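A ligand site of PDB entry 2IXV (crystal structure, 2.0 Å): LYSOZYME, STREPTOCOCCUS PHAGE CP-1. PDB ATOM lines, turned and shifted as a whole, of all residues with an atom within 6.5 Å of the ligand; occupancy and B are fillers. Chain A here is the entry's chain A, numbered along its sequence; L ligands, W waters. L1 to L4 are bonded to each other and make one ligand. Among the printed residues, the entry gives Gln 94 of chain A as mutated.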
ATOM      1  N   PHE A  61     -19.054 -13.617 -15.870  1.00  0.00           N
ATOM      2  CA  PHE A  61     -17.632 -13.691 -15.572  1.00  0.00           C
ATOM      3  C   PHE A  61     -17.302 -12.528 -14.649  1.00  0.00           C
ATOM      4  O   PHE A  61     -17.318 -11.375 -15.070  1.00  0.00           O
ATOM      5  CB  PHE A  61     -16.806 -13.593 -16.852  1.00  0.00           C
ATOM      6  CG  PHE A  61     -15.371 -14.002 -16.662  1.00  0.00           C
ATOM      7  CD1 PHE A  61     -14.981 -15.337 -16.808  1.00  0.00           C
ATOM      8  CD2 PHE A  61     -14.406 -13.064 -16.320  1.00  0.00           C
ATOM      9  CE1 PHE A  61     -13.656 -15.729 -16.603  1.00  0.00           C
ATOM     10  CE2 PHE A  61     -13.071 -13.442 -16.114  1.00  0.00           C
ATOM     11  CZ  PHE A  61     -12.701 -14.777 -16.259  1.00  0.00           C
ATOM     12  N   ASP A  92     -19.174 -16.906 -12.167  1.00  0.00           N
ATOM     13  CA  ASP A  92     -17.933 -17.481 -12.651  1.00  0.00           C
ATOM     14  C   ASP A  92     -16.808 -16.663 -12.020  1.00  0.00           C
ATOM     15  O   ASP A  92     -16.524 -15.556 -12.480  1.00  0.00           O
ATOM     16  CB  ASP A  92     -17.872 -17.387 -14.179  1.00  0.00           C
ATOM     17  CG  ASP A  92     -16.664 -18.082 -14.784  1.00  0.00           C
ATOM     18  OD1 ASP A  92     -15.570 -18.038 -14.187  1.00  0.00           O
ATOM     19  OD2 ASP A  92     -16.800 -18.669 -15.880  1.00  0.00           O
ATOM     20  N   GLN A  94     -13.029 -16.890 -11.384  1.00  0.00           N
ATOM     21  CA  GLN A  94     -11.801 -17.622 -11.645  1.00  0.00           C
ATOM     22  C   GLN A  94     -10.623 -16.745 -12.009  1.00  0.00           C
ATOM     23  O   GLN A  94      -9.582 -17.245 -12.444  1.00  0.00           O
ATOM     24  CB  GLN A  94     -12.048 -18.605 -12.786  1.00  0.00           C
ATOM     25  CG  GLN A  94     -12.213 -17.920 -14.130  1.00  0.00           C
ATOM     26  CD  GLN A  94     -12.460 -18.897 -15.263  1.00  0.00           C
ATOM     27  OE1 GLN A  94     -13.596 -19.292 -15.524  1.00  0.00           O
ATOM     28  NE2 GLN A  94     -11.395 -19.301 -15.936  1.00  0.00           N
ATOM     29  N   TYR A 125     -19.004 -20.941  -9.528  1.00  0.00           N
ATOM     30  CA  TYR A 125     -18.203 -21.744 -10.465  1.00  0.00           C
ATOM     31  C   TYR A 125     -16.734 -21.345 -10.345  1.00  0.00           C
ATOM     32  O   TYR A 125     -16.419 -20.164 -10.218  1.00  0.00           O
ATOM     33  CB  TYR A 125     -18.652 -21.500 -11.914  1.00  0.00           C
ATOM     34  CG  TYR A 125     -17.643 -22.016 -12.941  1.00  0.00           C
ATOM     35  CD1 TYR A 125     -17.660 -23.338 -13.361  1.00  0.00           C
ATOM     36  CD2 TYR A 125     -16.643 -21.181 -13.443  1.00  0.00           C
ATOM     37  CE1 TYR A 125     -16.706 -23.822 -14.259  1.00  0.00           C
ATOM     38  CE2 TYR A 125     -15.678 -21.651 -14.340  1.00  0.00           C
ATOM     39  CZ  TYR A 125     -15.714 -22.977 -14.731  1.00  0.00           C
ATOM     40  OH  TYR A 125     -14.747 -23.452 -15.586  1.00  0.00           O
ATOM     41  N   SER A 126     -15.849 -22.331 -10.411  1.00  0.00           N
ATOM     42  CA  SER A 126     -14.407 -22.093 -10.317  1.00  0.00           C
ATOM     43  C   SER A 126     -13.669 -23.431 -10.334  1.00  0.00           C
ATOM     44  O   SER A 126     -14.284 -24.471 -10.546  1.00  0.00           O
ATOM     45  CB  SER A 126     -14.084 -21.344  -9.011  1.00  0.00           C
ATOM     46  OG  SER A 126     -12.730 -20.936  -8.968  1.00  0.00           O
ATOM     47  N   TYR A 127     -12.357 -23.387 -10.136  1.00  0.00           N
ATOM     48  CA  TYR A 127     -11.587 -24.629 -10.064  1.00  0.00           C
ATOM     49  C   TYR A 127     -10.984 -24.721  -8.662  1.00  0.00           C
ATOM     50  O   TYR A 127     -10.833 -23.702  -7.975  1.00  0.00           O
ATOM     51  CB  TYR A 127     -10.536 -24.710 -11.188  1.00  0.00           C
ATOM     52  CG  TYR A 127      -9.531 -23.584 -11.295  1.00  0.00           C
ATOM     53  CD1 TYR A 127      -8.264 -23.704 -10.730  1.00  0.00           C
ATOM     54  CD2 TYR A 127      -9.825 -22.433 -12.021  1.00  0.00           C
ATOM     55  CE1 TYR A 127      -7.308 -22.708 -10.887  1.00  0.00           C
ATOM     56  CE2 TYR A 127      -8.880 -21.422 -12.190  1.00  0.00           C
ATOM     57  CZ  TYR A 127      -7.621 -21.571 -11.614  1.00  0.00           C
ATOM     58  OH  TYR A 127      -6.676 -20.588 -11.786  1.00  0.00           O
ATOM     59  N   LYS A 128     -10.685 -25.942  -8.224  1.00  0.00           N
ATOM     60  CA  LYS A 128     -10.181 -26.180  -6.870  1.00  0.00           C
ATOM     61  C   LYS A 128      -9.043 -25.320  -6.335  1.00  0.00           C
ATOM     62  O   LYS A 128      -9.229 -24.580  -5.371  1.00  0.00           O
ATOM     63  CB  LYS A 128      -9.839 -27.658  -6.689  1.00  0.00           C
ATOM     64  CG  LYS A 128      -9.587 -28.028  -5.238  1.00  0.00           C
ATOM     65  CD  LYS A 128      -9.494 -29.528  -5.045  1.00  0.00           C
ATOM     66  CE  LYS A 128      -9.401 -29.876  -3.567  1.00  0.00           C
ATOM     67  NZ  LYS A 128      -9.308 -31.343  -3.348  1.00  0.00           N
ATOM     68  N   PRO A 129      -7.841 -25.419  -6.920  1.00  0.00           N
ATOM     69  CA  PRO A 129      -6.752 -24.596  -6.393  1.00  0.00           C
ATOM     70  C   PRO A 129      -7.059 -23.095  -6.302  1.00  0.00           C
ATOM     71  O   PRO A 129      -6.701 -22.444  -5.325  1.00  0.00           O
ATOM     72  CB  PRO A 129      -5.584 -24.906  -7.332  1.00  0.00           C
ATOM     73  CG  PRO A 129      -6.245 -25.318  -8.595  1.00  0.00           C
ATOM     74  CD  PRO A 129      -7.397 -26.159  -8.121  1.00  0.00           C
ATOM     75  N   PHE A 130      -7.742 -22.550  -7.305  1.00  0.00           N
ATOM     76  CA  PHE A 130      -8.090 -21.133  -7.286  1.00  0.00           C
ATOM     77  C   PHE A 130      -8.962 -20.845  -6.075  1.00  0.00           C
ATOM     78  O   PHE A 130      -8.736 -19.889  -5.330  1.00  0.00           O
ATOM     79  CB  PHE A 130      -8.854 -20.727  -8.545  1.00  0.00           C
ATOM     80  CG  PHE A 130      -9.131 -19.243  -8.644  1.00  0.00           C
ATOM     81  CD1 PHE A 130      -8.172 -18.374  -9.146  1.00  0.00           C
ATOM     82  CD2 PHE A 130     -10.355 -18.729  -8.239  1.00  0.00           C
ATOM     83  CE1 PHE A 130      -8.426 -16.997  -9.238  1.00  0.00           C
ATOM     84  CE2 PHE A 130     -10.629 -17.361  -8.325  1.00  0.00           C
ATOM     85  CZ  PHE A 130      -9.659 -16.491  -8.827  1.00  0.00           C
ATOM     86  N   ALA A 151     -14.602 -27.060 -11.962  1.00  0.00           N
ATOM     87  CA  ALA A 151     -13.874 -27.520 -13.136  1.00  0.00           C
ATOM     88  C   ALA A 151     -12.656 -28.341 -12.723  1.00  0.00           C
ATOM     89  O   ALA A 151     -11.905 -27.942 -11.830  1.00  0.00           O
ATOM     90  CB  ALA A 151     -13.444 -26.331 -13.980  1.00  0.00           C
ATOM     91  N   GLY A 152     -12.481 -29.486 -13.374  1.00  0.00           N
ATOM     92  CA  GLY A 152     -11.350 -30.379 -13.129  1.00  0.00           C
ATOM     93  C   GLY A 152     -11.334 -31.274 -14.360  1.00  0.00           C
ATOM     94  O   GLY A 152     -12.180 -32.150 -14.501  1.00  0.00           O
ATOM     95  N   TYR A 153     -10.379 -31.037 -15.258  1.00  0.00           N
ATOM     96  CA  TYR A 153     -10.310 -31.771 -16.514  1.00  0.00           C
ATOM     97  C   TYR A 153      -9.467 -33.036 -16.578  1.00  0.00           C
ATOM     98  O   TYR A 153      -9.607 -33.823 -17.507  1.00  0.00           O
ATOM     99  CB  TYR A 153      -9.838 -30.824 -17.627  1.00  0.00           C
ATOM    100  CG  TYR A 153     -10.610 -29.516 -17.711  1.00  0.00           C
ATOM    101  CD1 TYR A 153     -10.033 -28.400 -18.302  1.00  0.00           C
ATOM    102  CD2 TYR A 153     -11.908 -29.415 -17.213  1.00  0.00           C
ATOM    103  CE1 TYR A 153     -10.733 -27.197 -18.397  1.00  0.00           C
ATOM    104  CE2 TYR A 153     -12.617 -28.206 -17.300  1.00  0.00           C
ATOM    105  CZ  TYR A 153     -12.020 -27.103 -17.893  1.00  0.00           C
ATOM    106  OH  TYR A 153     -12.689 -25.909 -17.970  1.00  0.00           O
ATOM    107  N   GLY A 154      -8.575 -33.237 -15.608  1.00  0.00           N
ATOM    108  CA  GLY A 154      -7.733 -34.418 -15.661  1.00  0.00           C
ATOM    109  C   GLY A 154      -6.833 -34.311 -16.887  1.00  0.00           C
ATOM    110  O   GLY A 154      -6.150 -33.297 -17.061  1.00  0.00           O
ATOM    111  N   LEU A 155      -6.843 -35.328 -17.732  1.00  0.00           N
ATOM    112  CA  LEU A 155      -6.030 -35.352 -18.955  1.00  0.00           C
ATOM    113  C   LEU A 155      -6.666 -34.442 -20.014  1.00  0.00           C
ATOM    114  O   LEU A 155      -6.041 -34.138 -21.041  1.00  0.00           O
ATOM    115  CB  LEU A 155      -5.942 -36.766 -19.522  1.00  0.00           C
ATOM    116  CG  LEU A 155      -5.301 -37.852 -18.644  1.00  0.00           C
ATOM    117  CD1 LEU A 155      -5.491 -39.210 -19.308  1.00  0.00           C
ATOM    118  CD2 LEU A 155      -3.836 -37.542 -18.442  1.00  0.00           C
ATOM    119  N   ASN A 156      -7.905 -34.030 -19.757  1.00  0.00           N
ATOM    120  CA  ASN A 156      -8.642 -33.155 -20.672  1.00  0.00           C
ATOM    121  C   ASN A 156      -8.715 -33.744 -22.072  1.00  0.00           C
ATOM    122  O   ASN A 156      -8.439 -33.068 -23.058  1.00  0.00           O
ATOM    123  CB  ASN A 156      -7.972 -31.780 -20.720  1.00  0.00           C
ATOM    124  CG  ASN A 156      -8.936 -30.672 -21.111  1.00  0.00           C
ATOM    125  OD1 ASN A 156      -8.529 -29.524 -21.316  1.00  0.00           O
ATOM    126  ND2 ASN A 156     -10.226 -30.998 -21.219  1.00  0.00           N
ATOM    127  N   TYR A 164      -9.846 -38.162 -11.790  1.00  0.00           N
ATOM    128  CA  TYR A 164      -9.548 -36.760 -11.505  1.00  0.00           C
ATOM    129  C   TYR A 164     -10.756 -35.954 -11.036  1.00  0.00           C
ATOM    130  O   TYR A 164     -10.800 -34.733 -11.218  1.00  0.00           O
ATOM    131  CB  TYR A 164      -8.945 -36.087 -12.740  1.00  0.00           C
ATOM    132  CG  TYR A 164      -7.660 -36.722 -13.192  1.00  0.00           C
ATOM    133  CD1 TYR A 164      -7.661 -37.789 -14.087  1.00  0.00           C
ATOM    134  CD2 TYR A 164      -6.433 -36.269 -12.700  1.00  0.00           C
ATOM    135  CE1 TYR A 164      -6.474 -38.398 -14.480  1.00  0.00           C
ATOM    136  CE2 TYR A 164      -5.235 -36.872 -13.086  1.00  0.00           C
ATOM    137  CZ  TYR A 164      -5.266 -37.940 -13.979  1.00  0.00           C
ATOM    138  OH  TYR A 164      -4.078 -38.537 -14.356  1.00  0.00           O
ATOM    139  N   GLN A 175     -17.534 -29.720 -14.444  1.00  0.00           N
ATOM    140  CA  GLN A 175     -17.077 -29.421 -15.790  1.00  0.00           C
ATOM    141  C   GLN A 175     -15.858 -30.319 -15.936  1.00  0.00           C
ATOM    142  O   GLN A 175     -14.769 -29.994 -15.467  1.00  0.00           O
ATOM    143  CB  GLN A 175     -16.673 -27.952 -15.888  1.00  0.00           C
ATOM    144  CG  GLN A 175     -16.517 -27.456 -17.312  1.00  0.00           C
ATOM    145  CD  GLN A 175     -16.097 -26.004 -17.335  1.00  0.00           C
ATOM    146  OE1 GLN A 175     -14.980 -25.673 -16.909  1.00  0.00           O
ATOM    147  NE2 GLN A 175     -16.980 -25.126 -17.804  1.00  0.00           N
ATOM    148  N   SER A 178     -12.718 -29.346 -21.420  1.00  0.00           N
ATOM    149  CA  SER A 178     -12.908 -28.177 -22.264  1.00  0.00           C
ATOM    150  C   SER A 178     -12.517 -28.575 -23.689  1.00  0.00           C
ATOM    151  O   SER A 178     -12.420 -27.751 -24.581  1.00  0.00           O
ATOM    152  CB  SER A 178     -12.002 -27.029 -21.792  1.00  0.00           C
ATOM    153  OG  SER A 178     -10.631 -27.417 -21.831  1.00  0.00           O
ATOM    154  N   ASP A 182     -16.616 -26.841 -23.569  1.00  0.00           N
ATOM    155  CA  ASP A 182     -16.890 -27.123 -22.168  1.00  0.00           C
ATOM    156  C   ASP A 182     -17.951 -28.185 -21.956  1.00  0.00           C
ATOM    157  O   ASP A 182     -19.091 -28.018 -22.373  1.00  0.00           O
ATOM    158  CB  ASP A 182     -17.295 -25.829 -21.433  1.00  0.00           C
ATOM    159  CG  ASP A 182     -16.127 -24.891 -21.225  1.00  0.00           C
ATOM    160  OD1 ASP A 182     -14.978 -25.311 -21.484  1.00  0.00           O
ATOM    161  OD2 ASP A 182     -16.355 -23.739 -20.791  1.00  0.00           O
HETATM  162  C1  LIG L   1      -7.863 -23.128 -15.950  1.00  0.00           C
HETATM  163  C2  LIG L   1      -7.946 -22.846 -17.466  1.00  0.00           C
HETATM  164  C3  LIG L   1      -9.157 -21.947 -17.713  1.00  0.00           C
HETATM  165  C4  LIG L   1     -10.413 -22.623 -17.211  1.00  0.00           C
HETATM  166  C5  LIG L   1     -10.271 -22.894 -15.718  1.00  0.00           C
HETATM  167  C6  LIG L   1     -11.460 -23.609 -15.125  1.00  0.00           C
HETATM  168  C7  LIG L   1      -5.661 -22.729 -18.281  1.00  0.00           C
HETATM  169  C8  LIG L   1      -4.471 -21.843 -18.602  1.00  0.00           C
HETATM  170  N1  LIG L   1      -6.767 -22.107 -17.863  1.00  0.00           N
HETATM  171  O1  LIG L   1      -9.283 -21.717 -19.111  1.00  0.00           O
HETATM  172  O2  LIG L   1     -11.532 -21.768 -17.440  1.00  0.00           O
HETATM  173  O3  LIG L   1      -9.093 -23.740 -15.499  1.00  0.00           O
HETATM  174  O4  LIG L   1     -12.377 -22.678 -14.586  1.00  0.00           O
HETATM  175  O5  LIG L   1      -5.573 -23.953 -18.402  1.00  0.00           O
HETATM  176  C1  LG2 L   2      -4.423 -25.510 -12.629  1.00  0.00           C
HETATM  177  C2  LG2 L   2      -5.874 -26.012 -12.671  1.00  0.00           C
HETATM  178  C3  LG2 L   2      -6.441 -25.763 -14.069  1.00  0.00           C
HETATM  179  C4  LG2 L   2      -6.342 -24.281 -14.419  1.00  0.00           C
HETATM  180  C5  LG2 L   2      -4.887 -23.847 -14.351  1.00  0.00           C
HETATM  181  C6  LG2 L   2      -4.744 -22.358 -14.645  1.00  0.00           C
HETATM  182  C7  LG2 L   2      -6.825 -27.956 -11.480  1.00  0.00           C
HETATM  183  C8  LG2 L   2      -6.728 -29.458 -11.209  1.00  0.00           C
HETATM  184  C9  LG2 L   2      -8.536 -27.037 -15.073  1.00  0.00           C
HETATM  185  C10 LG2 L   2      -7.977 -28.416 -15.077  1.00  0.00           C
HETATM  186  C11 LG2 L   2     -10.061 -26.944 -14.876  1.00  0.00           C
HETATM  187  O1  LG2 L   2      -3.610 -26.262 -13.518  1.00  0.00           O
HETATM  188  O2  LG2 L   2      -7.834 -26.213 -14.115  1.00  0.00           O
HETATM  189  O3  LG2 L   2      -6.853 -24.061 -15.746  1.00  0.00           O
HETATM  190  O4  LG2 L   2      -4.353 -24.112 -13.003  1.00  0.00           O
HETATM  191  O5  LG2 L   2      -3.379 -21.948 -14.567  1.00  0.00           O
HETATM  192  O6  LG2 L   2      -7.726 -27.293 -10.962  1.00  0.00           O
HETATM  193  O7  LG2 L   2      -8.306 -29.261 -14.224  1.00  0.00           O
HETATM  194  N1  LG2 L   2      -5.914 -27.437 -12.303  1.00  0.00           N
HETATM  195  N1  LG3 L   3      -7.117 -28.601 -16.089  1.00  0.00           N
HETATM  196  C1  LG3 L   3      -6.427 -29.863 -16.365  1.00  0.00           C
HETATM  197  C2  LG3 L   3      -5.366 -30.199 -15.322  1.00  0.00           C
HETATM  198  O1  LG3 L   3      -4.842 -29.300 -14.644  1.00  0.00           O
HETATM  199  C3  LG3 L   3      -5.774 -29.827 -17.742  1.00  0.00           C
HETATM  200  N1  LG4 L   4      -5.016 -31.491 -15.260  1.00  0.00           N
HETATM  201  C1  LG4 L   4      -3.951 -31.956 -14.370  1.00  0.00           C
HETATM  202  C2  LG4 L   4      -4.513 -32.503 -13.057  1.00  0.00           C
HETATM  203  O1  LG4 L   4      -5.475 -33.303 -13.088  1.00  0.00           O
HETATM  204  O2  LG4 L   4      -3.975 -32.113 -12.024  1.00  0.00           O
HETATM  205  C3  LG4 L   4      -3.049 -32.983 -15.050  1.00  0.00           C
HETATM  206  C4  LG4 L   4      -2.466 -32.426 -16.334  1.00  0.00           C
HETATM  207  C5  LG4 L   4      -1.561 -33.357 -17.087  1.00  0.00           C
HETATM  208  O3  LG4 L   4      -1.843 -33.578 -18.284  1.00  0.00           O
HETATM  209  N2  LG4 L   4      -0.591 -33.885 -16.499  1.00  0.00           N
HETATM  210  O   HOH W   1      -7.827 -31.943 -13.271  1.00  0.00           O
HETATM  211  O   HOH W   2      -9.992 -28.124  -9.976  1.00  0.00           O
HETATM  212  O   HOH W   3     -10.023 -24.218 -20.504  1.00  0.00           O
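OH of Tyr 125 lies within hydrogen-bond range of O4 of LIG L1.
The backbone carbonyl oxygen (O) of Gly 154 lies within hydrogen-bond range of a nitrogen (N1) of LG4 L4.
The side-chain amide nitrogen (NE2) of Gln 94 lies within hydrogen-bond range of an oxygen (O2) of LIG L1 (2.9 Å).
N of Tyr 153 is in hydrogen-bond range of O7 of LG2 L2 (2.9 Å).
The side-chain amide oxygen (OE1) of Gln 175 sits at hydrogen-bond distance from the side-chain hydroxyl (OH) of Tyr 125, 2.6 Å away.
The side-chain amide oxygen (OE1) of Gln 94 lies close to the side-chain carboxylate (OD1) of Asp 92 (2.7 Å).
The side-chain amide oxygen (OE1) of Gln 175 sits at hydrogen-bond distance from the side-chain hydroxyl (OH) of Tyr 153.
The backbone NH of Gly 152 is in hydrogen-bond range of the backbone carbonyl oxygen of Gln 175 (3.1 Å).
The backbone NH (N) of Ala 151 sits at hydrogen-bond distance from the backbone carbonyl oxygen (O) of Ser 126, 3.0 Å away.
CD2 of Tyr 127 touches O4 of LIG L1 (3.6 Å).
Pro 129 touches the ligand.
CB of Ala 151 touches C11 of LG2 L2 (3.6 Å).
CA of Gly 152 touches O7 of LG2 L2 (3.4 Å).
Tyr 164 touches the ligand.
Hydrophobic or aromatic side chains within 4 Å of the ligand: Tyr 125, Tyr 127, Pro 129, Ala 151, Tyr 153 and Tyr 164.
Within 4 Å of the ligand: Gln 94, Tyr 125, Tyr 127, Pro 129, Ala 151, Gly 152, Tyr 153, Gly 154 and Tyr 164.
The nearest printed residue that does not touch the ligand is Asn 156 (4.2 Å).
Water W2 lies within hydrogen-bond range of O6 of LG2 L2, O of Ala 151 and N of Lys 128.
Water W1 lies within hydrogen-bond range of O1 of LG4 L4 (2.7 Å), N of Gly 154 (2.8 Å) and N of Tyr 153 (3.4 Å).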
